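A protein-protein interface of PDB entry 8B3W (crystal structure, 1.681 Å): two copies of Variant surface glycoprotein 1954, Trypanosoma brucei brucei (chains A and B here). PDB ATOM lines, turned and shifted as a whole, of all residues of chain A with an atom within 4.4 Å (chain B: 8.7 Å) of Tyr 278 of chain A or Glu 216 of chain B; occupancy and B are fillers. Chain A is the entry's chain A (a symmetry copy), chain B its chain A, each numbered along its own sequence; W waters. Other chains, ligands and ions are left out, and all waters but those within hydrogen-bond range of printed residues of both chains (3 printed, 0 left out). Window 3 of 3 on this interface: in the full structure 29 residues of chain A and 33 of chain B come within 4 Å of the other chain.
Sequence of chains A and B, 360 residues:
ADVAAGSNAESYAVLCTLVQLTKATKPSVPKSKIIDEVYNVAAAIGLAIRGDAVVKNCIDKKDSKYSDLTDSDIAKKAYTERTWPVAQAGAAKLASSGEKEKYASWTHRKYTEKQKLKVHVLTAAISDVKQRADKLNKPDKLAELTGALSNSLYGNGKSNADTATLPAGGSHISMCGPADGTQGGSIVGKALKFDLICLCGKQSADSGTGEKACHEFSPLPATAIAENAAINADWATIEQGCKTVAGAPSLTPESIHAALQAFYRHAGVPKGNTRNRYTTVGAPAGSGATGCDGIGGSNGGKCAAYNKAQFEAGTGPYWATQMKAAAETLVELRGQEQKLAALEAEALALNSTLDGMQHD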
ATOM      1  N   GLY A 181      -7.845  -5.940 -18.490  1.00  0.00           N
ATOM      2  CA  GLY A 181      -6.818  -5.214 -19.227  1.00  0.00           C
ATOM      3  C   GLY A 181      -6.234  -3.992 -18.537  1.00  0.00           C
ATOM      4  O   GLY A 181      -5.481  -3.219 -19.162  1.00  0.00           O
ATOM      5  N   THR A 182      -6.544  -3.833 -17.240  1.00  0.00           N
ATOM      6  CA  THR A 182      -5.968  -2.792 -16.401  1.00  0.00           C
ATOM      7  C   THR A 182      -5.258  -3.307 -15.165  1.00  0.00           C
ATOM      8  O   THR A 182      -4.629  -2.500 -14.460  1.00  0.00           O
ATOM      9  CB  THR A 182      -7.063  -1.814 -15.926  1.00  0.00           C
ATOM     10  OG1 THR A 182      -7.898  -2.453 -14.929  1.00  0.00           O
ATOM     11  CG2 THR A 182      -7.905  -1.375 -17.101  1.00  0.00           C
ATOM     12  N   PRO A 270      -2.519   2.209 -26.111  1.00  0.00           N
ATOM     13  CA  PRO A 270      -3.396   1.063 -25.897  1.00  0.00           C
ATOM     14  C   PRO A 270      -3.343   0.078 -27.047  1.00  0.00           C
ATOM     15  O   PRO A 270      -3.208   0.449 -28.217  1.00  0.00           O
ATOM     16  CB  PRO A 270      -4.793   1.696 -25.765  1.00  0.00           C
ATOM     17  CG  PRO A 270      -4.509   3.044 -25.186  1.00  0.00           C
ATOM     18  CD  PRO A 270      -3.269   3.474 -25.966  1.00  0.00           C
ATOM     19  N   THR A 274      -9.496  -3.700 -30.090  1.00  0.00           N
ATOM     20  CA  THR A 274     -10.454  -2.687 -29.662  1.00  0.00           C
ATOM     21  C   THR A 274      -9.808  -1.646 -28.759  1.00  0.00           C
ATOM     22  O   THR A 274     -10.530  -0.864 -28.112  1.00  0.00           O
ATOM     23  CB  THR A 274     -11.655  -3.315 -28.959  1.00  0.00           C
ATOM     24  OG1 THR A 274     -11.236  -3.938 -27.736  1.00  0.00           O
ATOM     25  CG2 THR A 274     -12.349  -4.335 -29.868  1.00  0.00           C
ATOM     26  N   ARG A 275      -8.471  -1.621 -28.700  1.00  0.00           N
ATOM     27  CA  ARG A 275      -7.707  -0.641 -27.911  1.00  0.00           C
ATOM     28  C   ARG A 275      -8.105  -0.640 -26.427  1.00  0.00           C
ATOM     29  O   ARG A 275      -8.187   0.410 -25.780  1.00  0.00           O
ATOM     30  CB  ARG A 275      -7.849   0.746 -28.529  1.00  0.00           C
ATOM     31  CG  ARG A 275      -7.229   0.843 -29.924  1.00  0.00           C
ATOM     32  CD  ARG A 275      -7.827   2.003 -30.745  1.00  0.00           C
ATOM     33  NE  ARG A 275      -9.253   1.792 -30.937  1.00  0.00           N
ATOM     34  CZ  ARG A 275      -9.764   0.961 -31.835  1.00  0.00           C
ATOM     35  NH1 ARG A 275      -8.960   0.286 -32.644  1.00  0.00           N
ATOM     36  NH2 ARG A 275     -11.072   0.807 -31.933  1.00  0.00           N
ATOM     37  N   ASN A 276      -8.295  -1.831 -25.868  1.00  0.00           N
ATOM     38  CA  ASN A 276      -8.736  -2.013 -24.489  1.00  0.00           C
ATOM     39  C   ASN A 276      -7.673  -2.665 -23.589  1.00  0.00           C
ATOM     40  O   ASN A 276      -7.937  -2.906 -22.400  1.00  0.00           O
ATOM     41  CB  ASN A 276     -10.010  -2.858 -24.507  1.00  0.00           C
ATOM     42  CG  ASN A 276     -10.850  -2.675 -23.265  1.00  0.00           C
ATOM     43  OD1 ASN A 276     -11.059  -1.558 -22.770  1.00  0.00           O
ATOM     44  ND2 ASN A 276     -11.330  -3.778 -22.742  1.00  0.00           N
ATOM     45  N   ARG A 277      -6.469  -2.924 -24.106  1.00  0.00           N
ATOM     46  CA  ARG A 277      -5.365  -3.499 -23.319  1.00  0.00           C
ATOM     47  C   ARG A 277      -4.417  -2.367 -22.935  1.00  0.00           C
ATOM     48  O   ARG A 277      -3.651  -1.859 -23.768  1.00  0.00           O
ATOM     49  CB  ARG A 277      -4.645  -4.607 -24.096  1.00  0.00           C
ATOM     50  CG  ARG A 277      -5.607  -5.619 -24.793  1.00  0.00           C
ATOM     51  CD  ARG A 277      -6.687  -6.199 -23.868  1.00  0.00           C
ATOM     52  NE  ARG A 277      -6.109  -6.925 -22.734  1.00  0.00           N
ATOM     53  CZ  ARG A 277      -6.824  -7.512 -21.767  1.00  0.00           C
ATOM     54  NH1 ARG A 277      -8.167  -7.489 -21.809  1.00  0.00           N
ATOM     55  NH2 ARG A 277      -6.202  -8.146 -20.766  1.00  0.00           N
ATOM     56  N   TYR A 278      -4.492  -1.947 -21.669  1.00  0.00           N
ATOM     57  CA  TYR A 278      -3.765  -0.777 -21.202  1.00  0.00           C
ATOM     58  C   TYR A 278      -2.427  -1.161 -20.581  1.00  0.00           C
ATOM     59  O   TYR A 278      -2.255  -2.271 -20.054  1.00  0.00           O
ATOM     60  CB  TYR A 278      -4.606   0.002 -20.178  1.00  0.00           C
ATOM     61  CG  TYR A 278      -5.790   0.611 -20.814  1.00  0.00           C
ATOM     62  CD1 TYR A 278      -5.664   1.782 -21.514  1.00  0.00           C
ATOM     63  CD2 TYR A 278      -7.029  -0.018 -20.784  1.00  0.00           C
ATOM     64  CE1 TYR A 278      -6.748   2.350 -22.160  1.00  0.00           C
ATOM     65  CE2 TYR A 278      -8.122   0.540 -21.416  1.00  0.00           C
ATOM     66  CZ  TYR A 278      -7.973   1.729 -22.098  1.00  0.00           C
ATOM     67  OH  TYR A 278      -9.038   2.308 -22.733  1.00  0.00           O
ATOM     68  N   THR A 279      -1.494  -0.211 -20.639  1.00  0.00           N
ATOM     69  CA  THR A 279      -0.173  -0.287 -20.013  1.00  0.00           C
ATOM     70  C   THR A 279       0.428  -1.698 -20.128  1.00  0.00           C
ATOM     71  O   THR A 279       0.748  -2.374 -19.136  1.00  0.00           O
ATOM     72  CB  THR A 279      -0.234   0.206 -18.564  1.00  0.00           C
ATOM     73  OG1 THR A 279      -1.075  -0.648 -17.776  1.00  0.00           O
ATOM     74  CG2 THR A 279      -0.779   1.555 -18.497  1.00  0.00           C
ATOM     75  N   THR A 280       0.577  -2.133 -21.386  1.00  0.00           N
ATOM     76  CA  THR A 280       1.008  -3.505 -21.707  1.00  0.00           C
ATOM     77  C   THR A 280       2.115  -3.480 -22.755  1.00  0.00           C
ATOM     78  O   THR A 280       2.102  -2.634 -23.659  1.00  0.00           O
ATOM     79  CB  THR A 280      -0.192  -4.353 -22.207  1.00  0.00           C
ATOM     80  OG1 THR A 280      -1.112  -4.573 -21.124  1.00  0.00           O
ATOM     81  CG2 THR A 280       0.217  -5.742 -22.770  1.00  0.00           C
ATOM     82  N   LYS A 308      -2.271  -0.647 -14.387  1.00  0.00           N
ATOM     83  CA  LYS A 308      -2.579   0.660 -14.973  1.00  0.00           C
ATOM     84  C   LYS A 308      -2.534   1.776 -13.933  1.00  0.00           C
ATOM     85  O   LYS A 308      -1.963   2.851 -14.184  1.00  0.00           O
ATOM     86  CB  LYS A 308      -3.941   0.574 -15.660  1.00  0.00           C
ATOM     87  CG  LYS A 308      -4.463   1.906 -16.301  1.00  0.00           C
ATOM     88  CD  LYS A 308      -5.845   1.650 -16.930  1.00  0.00           C
ATOM     89  CE  LYS A 308      -6.394   2.860 -17.699  1.00  0.00           C
ATOM     90  NZ  LYS A 308      -6.963   3.842 -16.741  1.00  0.00           N
ATOM     91  N   ALA B   4     -10.413   7.109 -37.972  1.00  0.00           N
ATOM     92  CA  ALA B   4     -10.442   5.853 -37.239  1.00  0.00           C
ATOM     93  C   ALA B   4     -10.068   6.031 -35.770  1.00  0.00           C
ATOM     94  O   ALA B   4      -9.216   6.862 -35.406  1.00  0.00           O
ATOM     95  CB  ALA B   4      -9.511   4.866 -37.914  1.00  0.00           C
ATOM     96  N   ALA B   5     -10.727   5.254 -34.913  1.00  0.00           N
ATOM     97  CA  ALA B   5     -10.358   5.215 -33.498  1.00  0.00           C
ATOM     98  C   ALA B   5      -8.910   4.747 -33.363  1.00  0.00           C
ATOM     99  O   ALA B   5      -8.500   3.779 -34.010  1.00  0.00           O
ATOM    100  CB  ALA B   5     -11.284   4.276 -32.716  1.00  0.00           C
ATOM    101  N   GLY B   6      -8.136   5.443 -32.537  1.00  0.00           N
ATOM    102  CA  GLY B   6      -6.726   5.150 -32.325  1.00  0.00           C
ATOM    103  C   GLY B   6      -5.763   5.679 -33.384  1.00  0.00           C
ATOM    104  O   GLY B   6      -4.556   5.528 -33.208  1.00  0.00           O
ATOM    105  N   SER B   7      -6.254   6.320 -34.457  1.00  0.00           N
ATOM    106  CA  SER B   7      -5.384   6.738 -35.554  1.00  0.00           C
ATOM    107  C   SER B   7      -4.387   7.822 -35.170  1.00  0.00           C
ATOM    108  O   SER B   7      -3.392   7.996 -35.893  1.00  0.00           O
ATOM    109  CB  SER B   7      -6.199   7.247 -36.759  1.00  0.00           C
ATOM    110  OG  SER B   7      -7.125   8.290 -36.423  1.00  0.00           O
ATOM    111  N   ALA B   9      -3.123   7.824 -31.889  1.00  0.00           N
ATOM    112  CA  ALA B   9      -2.697   7.419 -30.547  1.00  0.00           C
ATOM    113  C   ALA B   9      -1.206   7.662 -30.305  1.00  0.00           C
ATOM    114  O   ALA B   9      -0.803   8.037 -29.196  1.00  0.00           O
ATOM    115  CB  ALA B   9      -3.023   5.944 -30.307  1.00  0.00           C
ATOM    116  N   TYR B  12      -0.631  11.298 -29.685  1.00  0.00           N
ATOM    117  CA  TYR B  12      -1.164  11.615 -28.356  1.00  0.00           C
ATOM    118  C   TYR B  12      -0.151  11.285 -27.251  1.00  0.00           C
ATOM    119  O   TYR B  12       0.133  12.117 -26.366  1.00  0.00           O
ATOM    120  CB  TYR B  12      -2.479  10.857 -28.192  1.00  0.00           C
ATOM    121  CG  TYR B  12      -3.208  11.089 -26.874  1.00  0.00           C
ATOM    122  CD1 TYR B  12      -3.622  12.371 -26.494  1.00  0.00           C
ATOM    123  CD2 TYR B  12      -3.512  10.036 -26.043  1.00  0.00           C
ATOM    124  CE1 TYR B  12      -4.283  12.578 -25.282  1.00  0.00           C
ATOM    125  CE2 TYR B  12      -4.194  10.224 -24.849  1.00  0.00           C
ATOM    126  CZ  TYR B  12      -4.573  11.476 -24.470  1.00  0.00           C
ATOM    127  OH  TYR B  12      -5.216  11.602 -23.260  1.00  0.00           O
ATOM    128  N   GLY B 208     -19.088   9.436 -33.035  1.00  0.00           N
ATOM    129  CA  GLY B 208     -18.725   8.505 -31.977  1.00  0.00           C
ATOM    130  C   GLY B 208     -17.378   7.831 -32.156  1.00  0.00           C
ATOM    131  O   GLY B 208     -16.844   7.263 -31.195  1.00  0.00           O
ATOM    132  N   THR B 209     -16.829   7.831 -33.359  1.00  0.00           N
ATOM    133  CA  THR B 209     -15.558   7.186 -33.649  1.00  0.00           C
ATOM    134  C   THR B 209     -14.406   8.170 -33.760  1.00  0.00           C
ATOM    135  O   THR B 209     -13.330   7.920 -33.216  1.00  0.00           O
ATOM    136  CB  THR B 209     -15.711   6.387 -34.945  1.00  0.00           C
ATOM    137  OG1 THR B 209     -16.713   5.394 -34.724  1.00  0.00           O
ATOM    138  CG2 THR B 209     -14.417   5.721 -35.377  1.00  0.00           C
ATOM    139  N   GLU B 211     -14.036  10.958 -32.339  1.00  0.00           N
ATOM    140  CA  GLU B 211     -13.705  11.490 -31.028  1.00  0.00           C
ATOM    141  C   GLU B 211     -12.746  10.581 -30.274  1.00  0.00           C
ATOM    142  O   GLU B 211     -12.213  10.988 -29.232  1.00  0.00           O
ATOM    143  CB  GLU B 211     -14.978  11.707 -30.203  1.00  0.00           C
ATOM    144  CG  GLU B 211     -15.960  12.679 -30.813  1.00  0.00           C
ATOM    145  CD  GLU B 211     -17.103  11.954 -31.520  1.00  0.00           C
ATOM    146  OE1 GLU B 211     -16.809  11.015 -32.302  1.00  0.00           O
ATOM    147  OE2 GLU B 211     -18.280  12.310 -31.281  1.00  0.00           O
ATOM    148  N   LYS B 212     -12.531   9.359 -30.767  1.00  0.00           N
ATOM    149  CA  LYS B 212     -11.550   8.442 -30.208  1.00  0.00           C
ATOM    150  C   LYS B 212     -10.286   8.334 -31.036  1.00  0.00           C
ATOM    151  O   LYS B 212      -9.520   7.384 -30.841  1.00  0.00           O
ATOM    152  CB  LYS B 212     -12.157   7.058 -30.059  1.00  0.00           C
ATOM    153  CG  LYS B 212     -13.377   7.058 -29.154  1.00  0.00           C
ATOM    154  CD  LYS B 212     -13.882   5.662 -28.896  1.00  0.00           C
ATOM    155  CE  LYS B 212     -14.784   5.179 -30.000  1.00  0.00           C
ATOM    156  NZ  LYS B 212     -15.360   3.843 -29.589  1.00  0.00           N
ATOM    157  N   ALA B 213     -10.046   9.283 -31.953  1.00  0.00           N
ATOM    158  CA  ALA B 213      -8.771   9.319 -32.675  1.00  0.00           C
ATOM    159  C   ALA B 213      -7.581   9.161 -31.728  1.00  0.00           C
ATOM    160  O   ALA B 213      -6.667   8.383 -32.009  1.00  0.00           O
ATOM    161  CB  ALA B 213      -8.642  10.623 -33.475  1.00  0.00           C
ATOM    162  N   CYS B 214      -7.551   9.916 -30.611  1.00  0.00           N
ATOM    163  CA  CYS B 214      -6.371   9.890 -29.748  1.00  0.00           C
ATOM    164  C   CYS B 214      -6.381   8.768 -28.714  1.00  0.00           C
ATOM    165  O   CYS B 214      -5.300   8.299 -28.299  1.00  0.00           O
ATOM    166  CB  CYS B 214      -6.195  11.221 -29.012  1.00  0.00           C
ATOM    167  SG  CYS B 214      -5.595  12.575 -30.009  1.00  0.00           S
ATOM    168  N   HIS B 215      -7.557   8.324 -28.293  1.00  0.00           N
ATOM    169  CA  HIS B 215      -7.680   7.561 -27.045  1.00  0.00           C
ATOM    170  C   HIS B 215      -9.138   7.155 -26.914  1.00  0.00           C
ATOM    171  O   HIS B 215     -10.024   7.804 -27.471  1.00  0.00           O
ATOM    172  CB  HIS B 215      -7.251   8.390 -25.823  1.00  0.00           C
ATOM    173  CG  HIS B 215      -7.044   7.580 -24.576  1.00  0.00           C
ATOM    174  ND1 HIS B 215      -6.028   6.657 -24.452  1.00  0.00           N
ATOM    175  CD2 HIS B 215      -7.705   7.574 -23.394  1.00  0.00           C
ATOM    176  CE1 HIS B 215      -6.085   6.104 -23.252  1.00  0.00           C
ATOM    177  NE2 HIS B 215      -7.091   6.644 -22.589  1.00  0.00           N
ATOM    178  N   GLU B 216      -9.384   6.097 -26.145  1.00  0.00           N
ATOM    179  CA  GLU B 216     -10.757   5.641 -25.913  1.00  0.00           C
ATOM    180  C   GLU B 216     -11.359   6.444 -24.751  1.00  0.00           C
ATOM    181  O   GLU B 216     -11.593   5.952 -23.646  1.00  0.00           O
ATOM    182  CB  GLU B 216     -10.783   4.141 -25.647  1.00  0.00           C
ATOM    183  CG  GLU B 216     -10.205   3.298 -26.792  1.00  0.00           C
ATOM    184  CD  GLU B 216     -11.138   3.173 -28.003  1.00  0.00           C
ATOM    185  OE1 GLU B 216     -12.303   2.739 -27.837  1.00  0.00           O
ATOM    186  OE2 GLU B 216     -10.698   3.481 -29.134  1.00  0.00           O
ATOM    187  N   PHE B 217     -11.584   7.718 -25.012  1.00  0.00           N
ATOM    188  CA  PHE B 217     -11.994   8.635 -23.955  1.00  0.00           C
ATOM    189  C   PHE B 217     -13.387   8.303 -23.438  1.00  0.00           C
ATOM    190  O   PHE B 217     -14.288   7.969 -24.207  1.00  0.00           O
ATOM    191  CB  PHE B 217     -12.008  10.075 -24.462  1.00  0.00           C
ATOM    192  CG  PHE B 217     -10.657  10.638 -24.763  1.00  0.00           C
ATOM    193  CD1 PHE B 217      -9.720  10.774 -23.757  1.00  0.00           C
ATOM    194  CD2 PHE B 217     -10.324  11.042 -26.051  1.00  0.00           C
ATOM    195  CE1 PHE B 217      -8.473  11.292 -24.018  1.00  0.00           C
ATOM    196  CE2 PHE B 217      -9.088  11.550 -26.308  1.00  0.00           C
ATOM    197  CZ  PHE B 217      -8.161  11.688 -25.290  1.00  0.00           C
ATOM    198  N   SER B 218     -13.568   8.419 -22.123  1.00  0.00           N
ATOM    199  CA  SER B 218     -14.915   8.481 -21.566  1.00  0.00           C
ATOM    200  C   SER B 218     -14.965   9.585 -20.518  1.00  0.00           C
ATOM    201  O   SER B 218     -14.141   9.597 -19.589  1.00  0.00           O
ATOM    202  CB  SER B 218     -15.334   7.162 -20.925  1.00  0.00           C
ATOM    203  OG  SER B 218     -16.708   7.213 -20.565  1.00  0.00           O
ATOM    204  N   PRO B 219     -15.870  10.555 -20.649  1.00  0.00           N
ATOM    205  CA  PRO B 219     -16.761  10.803 -21.791  1.00  0.00           C
ATOM    206  C   PRO B 219     -15.967  11.199 -23.041  1.00  0.00           C
ATOM    207  O   PRO B 219     -14.776  11.565 -22.960  1.00  0.00           O
ATOM    208  CB  PRO B 219     -17.666  11.954 -21.308  1.00  0.00           C
ATOM    209  CG  PRO B 219     -16.877  12.655 -20.292  1.00  0.00           C
ATOM    210  CD  PRO B 219     -15.896  11.647 -19.669  1.00  0.00           C
ATOM    211  N   LEU B 220     -16.601  11.040 -24.199  1.00  0.00           N
ATOM    212  CA  LEU B 220     -16.009  11.481 -25.448  1.00  0.00           C
ATOM    213  C   LEU B 220     -15.905  13.004 -25.469  1.00  0.00           C
ATOM    214  O   LEU B 220     -16.756  13.693 -24.900  1.00  0.00           O
ATOM    215  CB  LEU B 220     -16.863  11.031 -26.636  1.00  0.00           C
ATOM    216  CG  LEU B 220     -16.993   9.544 -26.984  1.00  0.00           C
ATOM    217  CD1 LEU B 220     -17.974   9.438 -28.125  1.00  0.00           C
ATOM    218  CD2 LEU B 220     -15.656   8.926 -27.374  1.00  0.00           C
ATOM    219  N   PRO B 221     -14.873  13.547 -26.116  1.00  0.00           N
ATOM    220  CA  PRO B 221     -14.875  14.979 -26.465  1.00  0.00           C
ATOM    221  C   PRO B 221     -16.172  15.332 -27.180  1.00  0.00           C
ATOM    222  O   PRO B 221     -16.569  14.664 -28.137  1.00  0.00           O
ATOM    223  CB  PRO B 221     -13.660  15.113 -27.389  1.00  0.00           C
ATOM    224  CG  PRO B 221     -12.734  14.051 -26.929  1.00  0.00           C
ATOM    225  CD  PRO B 221     -13.610  12.892 -26.493  1.00  0.00           C
ATOM    226  N   THR B 237     -10.784  16.320 -20.169  1.00  0.00           N
ATOM    227  CA  THR B 237     -10.794  14.901 -20.500  1.00  0.00           C
ATOM    228  C   THR B 237      -9.516  14.484 -21.225  1.00  0.00           C
ATOM    229  O   THR B 237      -8.897  13.461 -20.895  1.00  0.00           O
ATOM    230  CB  THR B 237     -12.022  14.602 -21.353  1.00  0.00           C
ATOM    231  OG1 THR B 237     -13.186  14.996 -20.613  1.00  0.00           O
ATOM    232  CG2 THR B 237     -12.078  13.120 -21.703  1.00  0.00           C
ATOM    233  N   GLY B 241      -6.221  11.921 -19.684  1.00  0.00           N
ATOM    234  CA  GLY B 241      -5.769  10.659 -20.247  1.00  0.00           C
ATOM    235  C   GLY B 241      -4.272  10.560 -20.451  1.00  0.00           C
ATOM    236  O   GLY B 241      -3.762   9.458 -20.684  1.00  0.00           O
ATOM    237  N   LYS B 243      -1.755  10.539 -18.492  1.00  0.00           N
ATOM    238  CA  LYS B 243      -1.041   9.642 -17.582  1.00  0.00           C
ATOM    239  C   LYS B 243      -1.190   8.179 -17.986  1.00  0.00           C
ATOM    240  O   LYS B 243      -0.295   7.368 -17.715  1.00  0.00           O
ATOM    241  CB  LYS B 243      -1.532   9.843 -16.156  1.00  0.00           C
ATOM    242  CG  LYS B 243      -3.030   9.719 -15.975  1.00  0.00           C
ATOM    243  CD  LYS B 243      -3.370   9.940 -14.477  1.00  0.00           C
ATOM    244  CE  LYS B 243      -4.832  10.020 -14.218  1.00  0.00           C
ATOM    245  NZ  LYS B 243      -5.366  11.293 -14.756  1.00  0.00           N
ATOM    246  N   THR B 244      -2.298   7.844 -18.663  1.00  0.00           N
ATOM    247  CA  THR B 244      -2.563   6.482 -19.084  1.00  0.00           C
ATOM    248  C   THR B 244      -1.632   6.078 -20.209  1.00  0.00           C
ATOM    249  O   THR B 244      -1.252   4.900 -20.298  1.00  0.00           O
ATOM    250  CB  THR B 244      -4.021   6.352 -19.537  1.00  0.00           C
ATOM    251  OG1 THR B 244      -4.853   6.800 -18.456  1.00  0.00           O
ATOM    252  CG2 THR B 244      -4.383   4.924 -19.934  1.00  0.00           C
ATOM    253  N   VAL B 245      -1.223   7.036 -21.048  1.00  0.00           N
ATOM    254  CA  VAL B 245      -0.457   6.708 -22.242  1.00  0.00           C
ATOM    255  C   VAL B 245       0.998   7.144 -22.164  1.00  0.00           C
ATOM    256  O   VAL B 245       1.792   6.696 -22.995  1.00  0.00           O
ATOM    257  CB  VAL B 245      -1.104   7.270 -23.536  1.00  0.00           C
ATOM    258  CG1 VAL B 245      -2.524   6.733 -23.732  1.00  0.00           C
ATOM    259  CG2 VAL B 245      -1.047   8.816 -23.633  1.00  0.00           C
HETATM  260  O   HOH W   1      -2.095   2.459 -21.535  1.00  0.00           O
HETATM  261  O   HOH W   2     -13.005   2.021 -30.156  1.00  0.00           O
HETATM  262  O   HOH W   3      -9.540   1.732 -35.429  1.00  0.00           O
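OE2 of Glu 216 of chain B is in salt-bridge range of NE of Arg 275 of chain A, 2.9 Å away.
No position is printed for both chains.
Of the 9 pairs that touch across the chains among the printed residues, none has its exchanged pair printed and touching as well.
Among the printed residues, pairs that only touch across the chains: Pro 270 of chain A with His 215 of chain B (3.9 Å), Arg 275 of chain A with Ala 5 of chain B (3.6 Å), Arg 275 of chain A with Gly 6 of chain B (3.7 Å), Tyr 278 of chain A with His 215 of chain B (3.97 Å), Tyr 278 of chain A with Glu 216 of chain B (3.9 Å), Tyr 278 of chain A with Thr 244 of chain B (3.7 Å), Thr 279 of chain A with Thr 244 of chain B (3.8 Å) and Lys 308 of chain A with Thr 244 of chain B (3.6 Å).
Water W2 lies within hydrogen-bond range of the side-chain carboxylate of Glu 216 of chain B (2.5 Å), the guanidinium group of Arg 275 of chain A (2.9 Å) and the side-chain amino group of Lys 212 of chain B (3.0 Å).
Water W3 bridges the backbone carbonyl oxygen of Ala 5 of chain B and the guanidinium group of Arg 275 of chain A.
Water W1 lies within hydrogen-bond range of O of Thr 244 of chain B (2.9 Å) and N of Thr 279 of chain A (2.9 Å).
The backbone carbonyl oxygen (O) of Tyr 278 of chain A lies within hydrogen-bond range of the side-chain hydroxyl (OG1) of Thr 280 of chain A (2.8 Å).
O of Lys 212 of chain B is in hydrogen-bond range of N of Gly 6 of chain B (2.9 Å).
N of Lys 308 of chain A is in hydrogen-bond range of O of Thr 182 of chain A (3.0 Å).
OE1 of Glu 216 of chain B is in salt-bridge range of NZ of Lys 212 of chain B.
N of Gly 6 of chain B lies close to O of Ala 213 of chain B (3.3 Å).
N of Tyr 278 of chain A sits at hydrogen-bond distance from O of Gly 181 of chain A (3.0 Å).
Of the printed residues of chain B, Pro 270 of chain A touches His 215.
Tyr 278 of chain A touches just these residues of chain B: His 215, Glu 216 and Thr 244.
Thr 279 of chain A touches one residue of chain B.
Printed residues of chain B within 4 Å of Lys 308 of chain A: Thr 244 (3.6 Å).
Printed residues of chain A within 4 Å of Ala 5 of chain B: Arg 275 (3.6 Å).
Ala 213 of chain B touches none of the printed residues of chain A.
Of the printed residues of chain A, His 215 of chain B touches Pro 270 and Tyr 278.
Of chain A, only Arg 275 (2.9 Å) and Tyr 278 (3.9 Å) come within 4 Å of Glu 216 of chain B.
Of the printed residues of chain A, Thr 244 of chain B touches Tyr 278, Thr 279 and Lys 308.
The nearest residue of chain B that does not touch Tyr 278 of chain A is Val 245 of chain B (6.3 Å).
The nearest residue of chain A that does not touch Glu 216 of chain B is Thr 274 of chain A (4.03 Å).
Of the 24 printed residues of chain B, 5 touch a printed residue of chain A.
Hydrophobic or aromatic side chains of chain B that line the printed part of chain A: Ala 5 and His 215.
Along chain B the printed residues that touch a printed residue of chain A span positions 5 to 244.
Printed residues of chain A that touch a printed residue of chain B: Pro 270, Arg 275, Tyr 278, Thr 279 and Lys 308.
Hydrophobic or aromatic side chains of chain A that line the printed part of chain B: Pro 270 and Tyr 278.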
